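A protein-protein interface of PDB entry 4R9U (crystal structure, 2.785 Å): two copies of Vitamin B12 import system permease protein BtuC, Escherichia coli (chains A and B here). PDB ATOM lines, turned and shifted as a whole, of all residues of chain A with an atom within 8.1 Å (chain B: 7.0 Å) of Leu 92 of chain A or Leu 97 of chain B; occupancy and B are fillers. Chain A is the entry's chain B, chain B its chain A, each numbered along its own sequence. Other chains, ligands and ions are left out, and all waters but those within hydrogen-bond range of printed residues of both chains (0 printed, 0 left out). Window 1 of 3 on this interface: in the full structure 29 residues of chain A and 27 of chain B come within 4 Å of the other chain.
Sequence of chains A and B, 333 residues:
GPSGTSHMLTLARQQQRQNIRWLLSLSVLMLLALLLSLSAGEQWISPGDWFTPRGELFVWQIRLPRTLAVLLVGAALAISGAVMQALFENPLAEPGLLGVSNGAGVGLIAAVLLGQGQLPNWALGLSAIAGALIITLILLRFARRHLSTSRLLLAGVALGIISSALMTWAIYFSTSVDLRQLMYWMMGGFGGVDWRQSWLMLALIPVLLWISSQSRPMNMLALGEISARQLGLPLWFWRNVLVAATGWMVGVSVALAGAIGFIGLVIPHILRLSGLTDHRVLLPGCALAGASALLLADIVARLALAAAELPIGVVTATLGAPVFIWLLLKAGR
ND2 of Asn 90 of chain B lies close to ND2 of Asn 90 of chain A, at 3.1 Å.
The backbone NH (N) of Leu 92 of chain B lies within hydrogen-bond range of the side-chain amide oxygen (OD1) of Asn 90 of chain B (2.7 Å). The backbone NH of Asn 90 of chain A lies within hydrogen-bond range of the backbone carbonyl oxygen of Gln 85 of chain A (3.1 Å). The side-chain amide oxygen of Gln 85 of chain A lies close to a ring nitrogen (ND1) of His 269 of chain A (3.4 Å). OD1 of Asn 90 of chain A is in hydrogen-bond range of N of Leu 92 of chain A. The backbone carbonyl oxygen (O) of Pro 91 of chain A lies within hydrogen-bond range of a ring nitrogen (NE2) of His 269 of chain A (2.8 Å).
Among the printed residues, merely in contact across the chains: Leu 92 of chain A with Leu 153 of chain B, Leu 153 of chain A with Leu 92 of chain B, His 269 of chain A with Leu 154 of chain B, Leu 92 of chain A with Leu 97 of chain B, Leu 92 of chain A with Val 157 of chain B, Val 157 of chain A with Leu 92 of chain B and Leu 97 of chain A with Leu 92 of chain B.
Of chain B, only Leu 97 (3.9 Å), Leu 153 (3.6 Å) and Val 157 (3.9 Å) come within 4 Å of Leu 92 of chain A. Printed residues of chain B within 4 Å of Val 157 of chain A: Leu 92 (3.9 Å). Printed residues of chain A within 4 Å of Leu 92 of chain B: Leu 97, Leu 153 and Val 157. Of chain A, only Leu 92 comes within 4 Å of Leu 97 of chain B. The nearest printed residue of chain A that does not touch Val 157 of chain B is Leu 265 of chain A (4.6 Å).
Of the 19 printed residues of chain A, 6 touch a printed residue of chain B. Hydrophobic or aromatic side chains of chain A that line the printed part of chain B: Leu 92, Leu 97, Leu 153, Val 157 and His 269. Hydrophobic or aromatic side chains of chain B that line the printed part of chain A: Leu 92, Leu 97, Leu 153, Leu 154 and Val 157. Among the printed residues, no Asp or Glu carboxylate lies within 4 Å of a Lys or Arg side-chain nitrogen of the other chain.
Asn 90 of chain B touches its own counterpart, Asn 90 of chain A. Leu 92 of chain A touches Leu 97 of chain B, and with the chains exchanged Leu 97 of chain A touches Leu 92 of chain B. Leu 92 of chain A touches Leu 153 of chain B, and with the chains exchanged Leu 153 of chain A touches Leu 92 of chain B. Leu 92 of chain A touches Val 157 of chain B, and with the chains exchanged Val 157 of chain A touches Leu 92 of chain B.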
ATOM      1  N   GLY A  81      15.769 -11.769  -5.905  1.00  0.00           N
ATOM      2  CA  GLY A  81      17.099 -11.720  -6.479  1.00  0.00           C
ATOM      3  C   GLY A  81      17.249 -10.534  -7.419  1.00  0.00           C
ATOM      4  O   GLY A  81      18.131  -9.696  -7.240  1.00  0.00           O
ATOM      5  N   MET A  84      17.104  -7.107  -5.596  1.00  0.00           N
ATOM      6  CA  MET A  84      18.301  -6.774  -4.819  1.00  0.00           C
ATOM      7  C   MET A  84      19.508  -6.491  -5.694  1.00  0.00           C
ATOM      8  O   MET A  84      20.216  -5.550  -5.464  1.00  0.00           O
ATOM      9  CB  MET A  84      18.645  -7.864  -3.837  1.00  0.00           C
ATOM     10  CG  MET A  84      17.661  -7.886  -2.697  1.00  0.00           C
ATOM     11  SD  MET A  84      17.747  -9.378  -1.693  1.00  0.00           S
ATOM     12  CE  MET A  84      18.913  -8.850  -0.442  1.00  0.00           C
ATOM     13  N   GLN A  85      19.768  -7.350  -6.664  1.00  0.00           N
ATOM     14  CA  GLN A  85      20.886  -7.139  -7.572  1.00  0.00           C
ATOM     15  C   GLN A  85      20.917  -5.756  -8.234  1.00  0.00           C
ATOM     16  O   GLN A  85      21.972  -5.220  -8.587  1.00  0.00           O
ATOM     17  CB  GLN A  85      20.866  -8.210  -8.659  1.00  0.00           C
ATOM     18  CG  GLN A  85      21.146  -9.562  -8.085  1.00  0.00           C
ATOM     19  CD  GLN A  85      21.330 -10.659  -9.103  1.00  0.00           C
ATOM     20  OE1 GLN A  85      21.523 -10.417 -10.300  1.00  0.00           O
ATOM     21  NE2 GLN A  85      21.321 -11.894  -8.616  1.00  0.00           N
ATOM     22  N   PHE A  88      21.328  -2.872  -4.921  1.00  0.00           N
ATOM     23  CA  PHE A  88      22.625  -2.797  -4.302  1.00  0.00           C
ATOM     24  C   PHE A  88      23.696  -2.649  -5.374  1.00  0.00           C
ATOM     25  O   PHE A  88      24.880  -2.492  -5.048  1.00  0.00           O
ATOM     26  CB  PHE A  88      22.855  -4.040  -3.475  1.00  0.00           C
ATOM     27  CG  PHE A  88      22.089  -4.044  -2.204  1.00  0.00           C
ATOM     28  CD1 PHE A  88      20.901  -4.728  -2.100  1.00  0.00           C
ATOM     29  CD2 PHE A  88      22.539  -3.328  -1.111  1.00  0.00           C
ATOM     30  CE1 PHE A  88      20.186  -4.711  -0.922  1.00  0.00           C
ATOM     31  CE2 PHE A  88      21.833  -3.306   0.063  1.00  0.00           C
ATOM     32  CZ  PHE A  88      20.657  -3.996   0.159  1.00  0.00           C
ATOM     33  N   GLU A  89      23.268  -2.699  -6.640  1.00  0.00           N
ATOM     34  CA  GLU A  89      24.154  -2.468  -7.788  1.00  0.00           C
ATOM     35  C   GLU A  89      25.255  -3.494  -7.857  1.00  0.00           C
ATOM     36  O   GLU A  89      26.387  -3.155  -8.156  1.00  0.00           O
ATOM     37  CB  GLU A  89      24.769  -1.067  -7.692  1.00  0.00           C
ATOM     38  CG  GLU A  89      23.919   0.083  -8.242  1.00  0.00           C
ATOM     39  CD  GLU A  89      24.479   1.479  -7.907  1.00  0.00           C
ATOM     40  OE1 GLU A  89      25.557   1.602  -7.272  1.00  0.00           O
ATOM     41  OE2 GLU A  89      23.812   2.465  -8.284  1.00  0.00           O
ATOM     42  N   ASN A  90      24.916  -4.752  -7.609  1.00  0.00           N
ATOM     43  CA  ASN A  90      25.920  -5.784  -7.425  1.00  0.00           C
ATOM     44  C   ASN A  90      25.436  -7.163  -7.869  1.00  0.00           C
ATOM     45  O   ASN A  90      24.414  -7.638  -7.376  1.00  0.00           O
ATOM     46  CB  ASN A  90      26.304  -5.836  -5.946  1.00  0.00           C
ATOM     47  CG  ASN A  90      27.352  -6.893  -5.648  1.00  0.00           C
ATOM     48  OD1 ASN A  90      27.238  -8.043  -6.071  1.00  0.00           O
ATOM     49  ND2 ASN A  90      28.333  -6.529  -4.827  1.00  0.00           N
ATOM     50  N   PRO A  91      26.211  -7.843  -8.728  1.00  0.00           N
ATOM     51  CA  PRO A  91      25.889  -9.166  -9.280  1.00  0.00           C
ATOM     52  C   PRO A  91      25.611 -10.263  -8.254  1.00  0.00           C
ATOM     53  O   PRO A  91      24.714 -11.074  -8.466  1.00  0.00           O
ATOM     54  CB  PRO A  91      27.125  -9.519 -10.076  1.00  0.00           C
ATOM     55  CG  PRO A  91      27.780  -8.217 -10.395  1.00  0.00           C
ATOM     56  CD  PRO A  91      27.516  -7.349  -9.207  1.00  0.00           C
ATOM     57  N   LEU A  92      26.415 -10.357  -7.216  1.00  0.00           N
ATOM     58  CA  LEU A  92      26.221 -11.356  -6.154  1.00  0.00           C
ATOM     59  C   LEU A  92      25.082 -11.121  -5.175  1.00  0.00           C
ATOM     60  O   LEU A  92      25.041 -11.788  -4.148  1.00  0.00           O
ATOM     61  CB  LEU A  92      27.492 -11.477  -5.326  1.00  0.00           C
ATOM     62  CG  LEU A  92      28.713 -11.759  -6.204  1.00  0.00           C
ATOM     63  CD1 LEU A  92      29.968 -12.120  -5.413  1.00  0.00           C
ATOM     64  CD2 LEU A  92      28.390 -12.837  -7.212  1.00  0.00           C
ATOM     65  N   ALA A  93      24.249 -10.096  -5.350  1.00  0.00           N
ATOM     66  CA  ALA A  93      23.170  -9.885  -4.402  1.00  0.00           C
ATOM     67  C   ALA A  93      22.241 -11.068  -4.543  1.00  0.00           C
ATOM     68  O   ALA A  93      21.815 -11.392  -5.650  1.00  0.00           O
ATOM     69  CB  ALA A  93      22.444  -8.553  -4.620  1.00  0.00           C
ATOM     70  N   GLU A  94      21.984 -11.741  -3.423  1.00  0.00           N
ATOM     71  CA  GLU A  94      21.149 -12.903  -3.352  1.00  0.00           C
ATOM     72  C   GLU A  94      19.988 -12.572  -2.401  1.00  0.00           C
ATOM     73  O   GLU A  94      19.860 -11.401  -1.983  1.00  0.00           O
ATOM     74  CB  GLU A  94      21.994 -14.059  -2.837  1.00  0.00           C
ATOM     75  CG  GLU A  94      21.942 -15.204  -3.725  1.00  0.00           C
ATOM     76  CD  GLU A  94      22.643 -16.356  -3.142  1.00  0.00           C
ATOM     77  OE1 GLU A  94      23.759 -16.182  -2.609  1.00  0.00           O
ATOM     78  OE2 GLU A  94      22.051 -17.450  -3.170  1.00  0.00           O
ATOM     79  N   PRO A  95      19.134 -13.562  -2.051  1.00  0.00           N
ATOM     80  CA  PRO A  95      18.208 -13.065  -1.037  1.00  0.00           C
ATOM     81  C   PRO A  95      18.639 -13.373   0.424  1.00  0.00           C
ATOM     82  O   PRO A  95      18.414 -12.584   1.379  1.00  0.00           O
ATOM     83  CB  PRO A  95      16.892 -13.765  -1.411  1.00  0.00           C
ATOM     84  CG  PRO A  95      17.257 -15.016  -2.112  1.00  0.00           C
ATOM     85  CD  PRO A  95      18.693 -14.870  -2.595  1.00  0.00           C
ATOM     86  N   GLY A  96      19.259 -14.536   0.603  1.00  0.00           N
ATOM     87  CA  GLY A  96      19.722 -14.886   1.930  1.00  0.00           C
ATOM     88  C   GLY A  96      21.054 -14.223   2.230  1.00  0.00           C
ATOM     89  O   GLY A  96      21.946 -14.828   2.823  1.00  0.00           O
ATOM     90  N   LEU A  97      21.193 -12.965   1.817  1.00  0.00           N
ATOM     91  CA  LEU A  97      22.473 -12.303   1.977  1.00  0.00           C
ATOM     92  C   LEU A  97      22.407 -11.176   3.002  1.00  0.00           C
ATOM     93  O   LEU A  97      23.430 -10.724   3.518  1.00  0.00           O
ATOM     94  CB  LEU A  97      22.953 -11.795   0.621  1.00  0.00           C
ATOM     95  CG  LEU A  97      24.123 -10.812   0.608  1.00  0.00           C
ATOM     96  CD1 LEU A  97      25.393 -11.624   0.795  1.00  0.00           C
ATOM     97  CD2 LEU A  97      24.168 -10.008  -0.676  1.00  0.00           C
ATOM     98  N   LEU A 153      24.911  -2.328   2.362  1.00  0.00           N
ATOM     99  CA  LEU A 153      25.085  -3.716   1.966  1.00  0.00           C
ATOM    100  C   LEU A 153      26.017  -4.362   2.961  1.00  0.00           C
ATOM    101  O   LEU A 153      25.644  -5.372   3.547  1.00  0.00           O
ATOM    102  CB  LEU A 153      25.637  -3.839   0.538  1.00  0.00           C
ATOM    103  CG  LEU A 153      25.731  -5.190  -0.175  1.00  0.00           C
ATOM    104  CD1 LEU A 153      26.076  -4.922  -1.619  1.00  0.00           C
ATOM    105  CD2 LEU A 153      26.787  -6.105   0.397  1.00  0.00           C
ATOM    106  N   VAL A 157      25.282  -7.620   5.290  1.00  0.00           N
ATOM    107  CA  VAL A 157      26.001  -8.883   5.235  1.00  0.00           C
ATOM    108  C   VAL A 157      26.406  -9.276   6.643  1.00  0.00           C
ATOM    109  O   VAL A 157      26.255 -10.432   7.075  1.00  0.00           O
ATOM    110  CB  VAL A 157      27.254  -8.793   4.385  1.00  0.00           C
ATOM    111  CG1 VAL A 157      28.014 -10.070   4.472  1.00  0.00           C
ATOM    112  CG2 VAL A 157      26.905  -8.485   2.973  1.00  0.00           C
ATOM    113  N   GLY A 264      17.450 -17.327  -6.498  1.00  0.00           N
ATOM    114  CA  GLY A 264      17.470 -15.877  -6.486  1.00  0.00           C
ATOM    115  C   GLY A 264      18.876 -15.351  -6.684  1.00  0.00           C
ATOM    116  O   GLY A 264      19.255 -14.362  -6.081  1.00  0.00           O
ATOM    117  N   LEU A 265      19.642 -15.997  -7.554  1.00  0.00           N
ATOM    118  CA  LEU A 265      21.017 -15.616  -7.804  1.00  0.00           C
ATOM    119  C   LEU A 265      21.314 -15.925  -9.245  1.00  0.00           C
ATOM    120  O   LEU A 265      21.783 -15.080  -9.999  1.00  0.00           O
ATOM    121  CB  LEU A 265      21.986 -16.366  -6.903  1.00  0.00           C
ATOM    122  CG  LEU A 265      23.468 -16.096  -7.222  1.00  0.00           C
ATOM    123  CD1 LEU A 265      23.806 -14.601  -7.204  1.00  0.00           C
ATOM    124  CD2 LEU A 265      24.408 -16.863  -6.304  1.00  0.00           C
ATOM    125  N   HIS A 269      20.379 -13.804 -13.290  1.00  0.00           N
ATOM    126  CA  HIS A 269      21.565 -13.541 -14.105  1.00  0.00           C
ATOM    127  C   HIS A 269      21.379 -14.135 -15.486  1.00  0.00           C
ATOM    128  O   HIS A 269      21.670 -13.488 -16.490  1.00  0.00           O
ATOM    129  CB  HIS A 269      22.814 -14.100 -13.448  1.00  0.00           C
ATOM    130  CG  HIS A 269      23.518 -13.103 -12.594  1.00  0.00           C
ATOM    131  ND1 HIS A 269      23.408 -11.744 -12.807  1.00  0.00           N
ATOM    132  CD2 HIS A 269      24.286 -13.257 -11.491  1.00  0.00           C
ATOM    133  CE1 HIS A 269      24.104 -11.103 -11.888  1.00  0.00           C
ATOM    134  NE2 HIS A 269      24.646 -11.997 -11.079  1.00  0.00           N
ATOM    135  N   ARG A 272      19.186 -12.219 -17.762  1.00  0.00           N
ATOM    136  CA  ARG A 272      19.848 -11.036 -18.303  1.00  0.00           C
ATOM    137  C   ARG A 272      20.831 -11.413 -19.403  1.00  0.00           C
ATOM    138  O   ARG A 272      20.960 -10.680 -20.377  1.00  0.00           O
ATOM    139  CB  ARG A 272      20.588 -10.257 -17.215  1.00  0.00           C
ATOM    140  CG  ARG A 272      19.953  -8.937 -16.818  1.00  0.00           C
ATOM    141  CD  ARG A 272      20.571  -8.454 -15.536  1.00  0.00           C
ATOM    142  NE  ARG A 272      19.897  -9.052 -14.395  1.00  0.00           N
ATOM    143  CZ  ARG A 272      20.302  -8.909 -13.144  1.00  0.00           C
ATOM    144  NH1 ARG A 272      21.391  -8.205 -12.889  1.00  0.00           N
ATOM    145  NH2 ARG A 272      19.632  -9.482 -12.154  1.00  0.00           N
ATOM    146  N   MET B  84      41.558 -10.043  -4.066  1.00  0.00           N
ATOM    147  CA  MET B  84      40.382 -10.333  -4.870  1.00  0.00           C
ATOM    148  C   MET B  84      39.374  -9.217  -4.906  1.00  0.00           C
ATOM    149  O   MET B  84      38.779  -8.983  -5.932  1.00  0.00           O
ATOM    150  CB  MET B  84      39.720 -11.581  -4.410  1.00  0.00           C
ATOM    151  CG  MET B  84      40.550 -12.753  -4.795  1.00  0.00           C
ATOM    152  SD  MET B  84      39.978 -14.220  -3.981  1.00  0.00           S
ATOM    153  CE  MET B  84      38.818 -14.809  -5.227  1.00  0.00           C
ATOM    154  N   PHE B  88      38.411  -7.899  -8.693  1.00  0.00           N
ATOM    155  CA  PHE B  88      37.075  -8.101  -9.210  1.00  0.00           C
ATOM    156  C   PHE B  88      36.245  -6.848  -9.003  1.00  0.00           C
ATOM    157  O   PHE B  88      35.074  -6.795  -9.415  1.00  0.00           O
ATOM    158  CB  PHE B  88      36.412  -9.286  -8.531  1.00  0.00           C
ATOM    159  CG  PHE B  88      36.924 -10.605  -8.998  1.00  0.00           C
ATOM    160  CD1 PHE B  88      37.765 -11.354  -8.203  1.00  0.00           C
ATOM    161  CD2 PHE B  88      36.529 -11.115 -10.221  1.00  0.00           C
ATOM    162  CE1 PHE B  88      38.227 -12.577  -8.638  1.00  0.00           C
ATOM    163  CE2 PHE B  88      36.987 -12.324 -10.662  1.00  0.00           C
ATOM    164  CZ  PHE B  88      37.832 -13.059  -9.872  1.00  0.00           C
ATOM    165  N   ASN B  90      34.870  -5.546  -6.428  1.00  0.00           N
ATOM    166  CA  ASN B  90      33.630  -5.898  -5.734  1.00  0.00           C
ATOM    167  C   ASN B  90      33.849  -6.244  -4.266  1.00  0.00           C
ATOM    168  O   ASN B  90      34.596  -7.181  -3.958  1.00  0.00           O
ATOM    169  CB  ASN B  90      32.965  -7.102  -6.399  1.00  0.00           C
ATOM    170  CG  ASN B  90      31.664  -7.518  -5.704  1.00  0.00           C
ATOM    171  OD1 ASN B  90      31.614  -7.688  -4.483  1.00  0.00           O
ATOM    172  ND2 ASN B  90      30.622  -7.755  -6.501  1.00  0.00           N
ATOM    173  N   LEU B  92      32.059  -7.909  -1.841  1.00  0.00           N
ATOM    174  CA  LEU B  92      31.809  -9.308  -1.444  1.00  0.00           C
ATOM    175  C   LEU B  92      32.804 -10.334  -1.943  1.00  0.00           C
ATOM    176  O   LEU B  92      32.549 -11.530  -1.822  1.00  0.00           O
ATOM    177  CB  LEU B  92      30.425  -9.740  -1.930  1.00  0.00           C
ATOM    178  CG  LEU B  92      29.267  -8.849  -1.463  1.00  0.00           C
ATOM    179  CD1 LEU B  92      27.900  -9.435  -1.770  1.00  0.00           C
ATOM    180  CD2 LEU B  92      29.377  -8.649   0.003  1.00  0.00           C
ATOM    181  N   ALA B  93      33.859  -9.924  -2.644  1.00  0.00           N
ATOM    182  CA  ALA B  93      34.830 -10.887  -3.112  1.00  0.00           C
ATOM    183  C   ALA B  93      35.511 -11.423  -1.876  1.00  0.00           C
ATOM    184  O   ALA B  93      36.027 -10.663  -1.055  1.00  0.00           O
ATOM    185  CB  ALA B  93      35.816 -10.278  -4.106  1.00  0.00           C
ATOM    186  N   GLU B  94      35.462 -12.742  -1.737  1.00  0.00           N
ATOM    187  CA  GLU B  94      35.997 -13.464  -0.628  1.00  0.00           C
ATOM    188  C   GLU B  94      37.071 -14.372  -1.226  1.00  0.00           C
ATOM    189  O   GLU B  94      37.415 -14.205  -2.418  1.00  0.00           O
ATOM    190  CB  GLU B  94      34.859 -14.241   0.023  1.00  0.00           C
ATOM    191  CG  GLU B  94      34.751 -13.970   1.454  1.00  0.00           C
ATOM    192  CD  GLU B  94      33.723 -14.823   2.100  1.00  0.00           C
ATOM    193  OE1 GLU B  94      32.609 -14.964   1.553  1.00  0.00           O
ATOM    194  OE2 GLU B  94      34.042 -15.399   3.157  1.00  0.00           O
ATOM    195  N   PRO B  95      37.638 -15.301  -0.431  1.00  0.00           N
ATOM    196  CA  PRO B  95      38.507 -16.157  -1.230  1.00  0.00           C
ATOM    197  C   PRO B  95      37.803 -17.456  -1.725  1.00  0.00           C
ATOM    198  O   PRO B  95      38.035 -17.954  -2.859  1.00  0.00           O
ATOM    199  CB  PRO B  95      39.673 -16.445  -0.269  1.00  0.00           C
ATOM    200  CG  PRO B  95      39.135 -16.316   1.110  1.00  0.00           C
ATOM    201  CD  PRO B  95      37.845 -15.514   1.019  1.00  0.00           C
ATOM    202  N   GLY B  96      36.933 -17.993  -0.868  1.00  0.00           N
ATOM    203  CA  GLY B  96      36.212 -19.206  -1.213  1.00  0.00           C
ATOM    204  C   GLY B  96      35.005 -18.937  -2.086  1.00  0.00           C
ATOM    205  O   GLY B  96      33.944 -19.540  -1.934  1.00  0.00           O
ATOM    206  N   LEU B  97      35.175 -18.028  -3.035  1.00  0.00           N
ATOM    207  CA  LEU B  97      34.042 -17.624  -3.832  1.00  0.00           C
ATOM    208  C   LEU B  97      34.170 -18.097  -5.287  1.00  0.00           C
ATOM    209  O   LEU B  97      33.183 -18.159  -6.024  1.00  0.00           O
ATOM    210  CB  LEU B  97      33.899 -16.109  -3.725  1.00  0.00           C
ATOM    211  CG  LEU B  97      32.997 -15.335  -4.685  1.00  0.00           C
ATOM    212  CD1 LEU B  97      31.545 -15.424  -4.221  1.00  0.00           C
ATOM    213  CD2 LEU B  97      33.454 -13.898  -4.823  1.00  0.00           C
ATOM    214  N   LEU B  98      35.372 -18.491  -5.684  1.00  0.00           N
ATOM    215  CA  LEU B  98      35.575 -18.998  -7.038  1.00  0.00           C
ATOM    216  C   LEU B  98      35.722 -20.506  -7.029  1.00  0.00           C
ATOM    217  O   LEU B  98      36.139 -21.091  -8.020  1.00  0.00           O
ATOM    218  CB  LEU B  98      36.806 -18.376  -7.706  1.00  0.00           C
ATOM    219  CG  LEU B  98      36.908 -16.850  -7.766  1.00  0.00           C
ATOM    220  CD1 LEU B  98      37.963 -16.415  -8.780  1.00  0.00           C
ATOM    221  CD2 LEU B  98      35.555 -16.224  -8.075  1.00  0.00           C
ATOM    222  N   GLY B  99      35.391 -21.148  -5.915  1.00  0.00           N
ATOM    223  CA  GLY B  99      35.410 -22.595  -5.892  1.00  0.00           C
ATOM    224  C   GLY B  99      36.696 -23.243  -5.440  1.00  0.00           C
ATOM    225  O   GLY B  99      36.675 -24.394  -5.013  1.00  0.00           O
ATOM    226  N   VAL B 100      37.811 -22.543  -5.571  1.00  0.00           N
ATOM    227  CA  VAL B 100      39.090 -23.037  -5.080  1.00  0.00           C
ATOM    228  C   VAL B 100      39.012 -23.709  -3.681  1.00  0.00           C
ATOM    229  O   VAL B 100      39.415 -24.862  -3.523  1.00  0.00           O
ATOM    230  CB  VAL B 100      40.102 -21.888  -5.093  1.00  0.00           C
ATOM    231  CG1 VAL B 100      39.511 -20.630  -4.397  1.00  0.00           C
ATOM    232  CG2 VAL B 100      41.381 -22.334  -4.412  1.00  0.00           C
ATOM    233  N   SER B 101      38.376 -23.019  -2.723  1.00  0.00           N
ATOM    234  CA  SER B 101      38.176 -23.550  -1.386  1.00  0.00           C
ATOM    235  C   SER B 101      37.385 -24.849  -1.431  1.00  0.00           C
ATOM    236  O   SER B 101      37.705 -25.784  -0.714  1.00  0.00           O
ATOM    237  CB  SER B 101      37.413 -22.529  -0.512  1.00  0.00           C
ATOM    238  OG  SER B 101      37.670 -22.679   0.876  1.00  0.00           O
ATOM    239  N   LEU B 153      34.054 -13.408 -12.961  1.00  0.00           N
ATOM    240  CA  LEU B 153      33.620 -13.588 -11.582  1.00  0.00           C
ATOM    241  C   LEU B 153      32.454 -14.527 -11.514  1.00  0.00           C
ATOM    242  O   LEU B 153      32.466 -15.451 -10.719  1.00  0.00           O
ATOM    243  CB  LEU B 153      33.248 -12.254 -10.954  1.00  0.00           C
ATOM    244  CG  LEU B 153      32.835 -12.158  -9.486  1.00  0.00           C
ATOM    245  CD1 LEU B 153      32.920 -10.725  -9.066  1.00  0.00           C
ATOM    246  CD2 LEU B 153      31.430 -12.689  -9.211  1.00  0.00           C
ATOM    247  N   LEU B 154      31.440 -14.235 -12.330  1.00  0.00           N
ATOM    248  CA  LEU B 154      30.209 -15.023 -12.420  1.00  0.00           C
ATOM    249  C   LEU B 154      30.528 -16.471 -12.745  1.00  0.00           C
ATOM    250  O   LEU B 154      30.048 -17.395 -12.070  1.00  0.00           O
ATOM    251  CB  LEU B 154      29.247 -14.417 -13.465  1.00  0.00           C
ATOM    252  CG  LEU B 154      28.382 -13.286 -12.877  1.00  0.00           C
ATOM    253  CD1 LEU B 154      27.190 -12.859 -13.742  1.00  0.00           C
ATOM    254  CD2 LEU B 154      27.905 -13.758 -11.521  1.00  0.00           C
ATOM    255  N   ALA B 155      31.390 -16.653 -13.744  1.00  0.00           N
ATOM    256  CA  ALA B 155      31.850 -17.980 -14.106  1.00  0.00           C
ATOM    257  C   ALA B 155      32.487 -18.669 -12.902  1.00  0.00           C
ATOM    258  O   ALA B 155      32.200 -19.829 -12.634  1.00  0.00           O
ATOM    259  CB  ALA B 155      32.836 -17.895 -15.250  1.00  0.00           C
ATOM    260  N   GLY B 156      33.307 -17.950 -12.151  1.00  0.00           N
ATOM    261  CA  GLY B 156      33.916 -18.515 -10.956  1.00  0.00           C
ATOM    262  C   GLY B 156      32.932 -18.925  -9.866  1.00  0.00           C
ATOM    263  O   GLY B 156      33.095 -19.981  -9.244  1.00  0.00           O
ATOM    264  N   VAL B 157      31.947 -18.067  -9.605  1.00  0.00           N
ATOM    265  CA  VAL B 157      30.919 -18.333  -8.613  1.00  0.00           C
ATOM    266  C   VAL B 157      30.239 -19.621  -8.992  1.00  0.00           C
ATOM    267  O   VAL B 157      30.011 -20.507  -8.163  1.00  0.00           O
ATOM    268  CB  VAL B 157      29.884 -17.189  -8.555  1.00  0.00           C
ATOM    269  CG1 VAL B 157      28.699 -17.541  -7.663  1.00  0.00           C
ATOM    270  CG2 VAL B 157      30.550 -15.913  -8.107  1.00  0.00           C
ATOM    271  N   ALA B 158      29.964 -19.713 -10.291  1.00  0.00           N
ATOM    272  CA  ALA B 158      29.336 -20.886 -10.859  1.00  0.00           C
ATOM    273  C   ALA B 158      30.179 -22.154 -10.656  1.00  0.00           C
ATOM    274  O   ALA B 158      29.641 -23.177 -10.237  1.00  0.00           O
ATOM    275  CB  ALA B 158      29.053 -20.654 -12.330  1.00  0.00           C
ATOM    276  N   LEU B 159      31.489 -22.082 -10.919  1.00  0.00           N
ATOM    277  CA  LEU B 159      32.396 -23.199 -10.613  1.00  0.00           C
ATOM    278  C   LEU B 159      32.260 -23.609  -9.171  1.00  0.00           C
ATOM    279  O   LEU B 159      32.190 -24.800  -8.847  1.00  0.00           O
ATOM    280  CB  LEU B 159      33.853 -22.836 -10.870  1.00  0.00           C
ATOM    281  CG  LEU B 159      34.452 -23.204 -12.215  1.00  0.00           C
ATOM    282  CD1 LEU B 159      35.979 -23.231 -12.165  1.00  0.00           C
ATOM    283  CD2 LEU B 159      33.890 -24.544 -12.586  1.00  0.00           C
ATOM    284  N   GLY B 160      32.210 -22.631  -8.290  1.00  0.00           N
ATOM    285  CA  GLY B 160      32.133 -22.954  -6.883  1.00  0.00           C
ATOM    286  C   GLY B 160      30.844 -23.703  -6.590  1.00  0.00           C
ATOM    287  O   GLY B 160      30.844 -24.681  -5.833  1.00  0.00           O
ATOM    288  N   ILE B 161      29.765 -23.265  -7.246  1.00  0.00           N
ATOM    289  CA  ILE B 161      28.454 -23.875  -7.064  1.00  0.00           C
ATOM    290  C   ILE B 161      28.475 -25.343  -7.491  1.00  0.00           C
ATOM    291  O   ILE B 161      27.965 -26.207  -6.769  1.00  0.00           O
ATOM    292  CB  ILE B 161      27.363 -23.094  -7.816  1.00  0.00           C
ATOM    293  CG1 ILE B 161      27.214 -21.691  -7.220  1.00  0.00           C
ATOM    294  CG2 ILE B 161      26.051 -23.817  -7.717  1.00  0.00           C
ATOM    295  CD1 ILE B 161      26.149 -20.851  -7.895  1.00  0.00           C
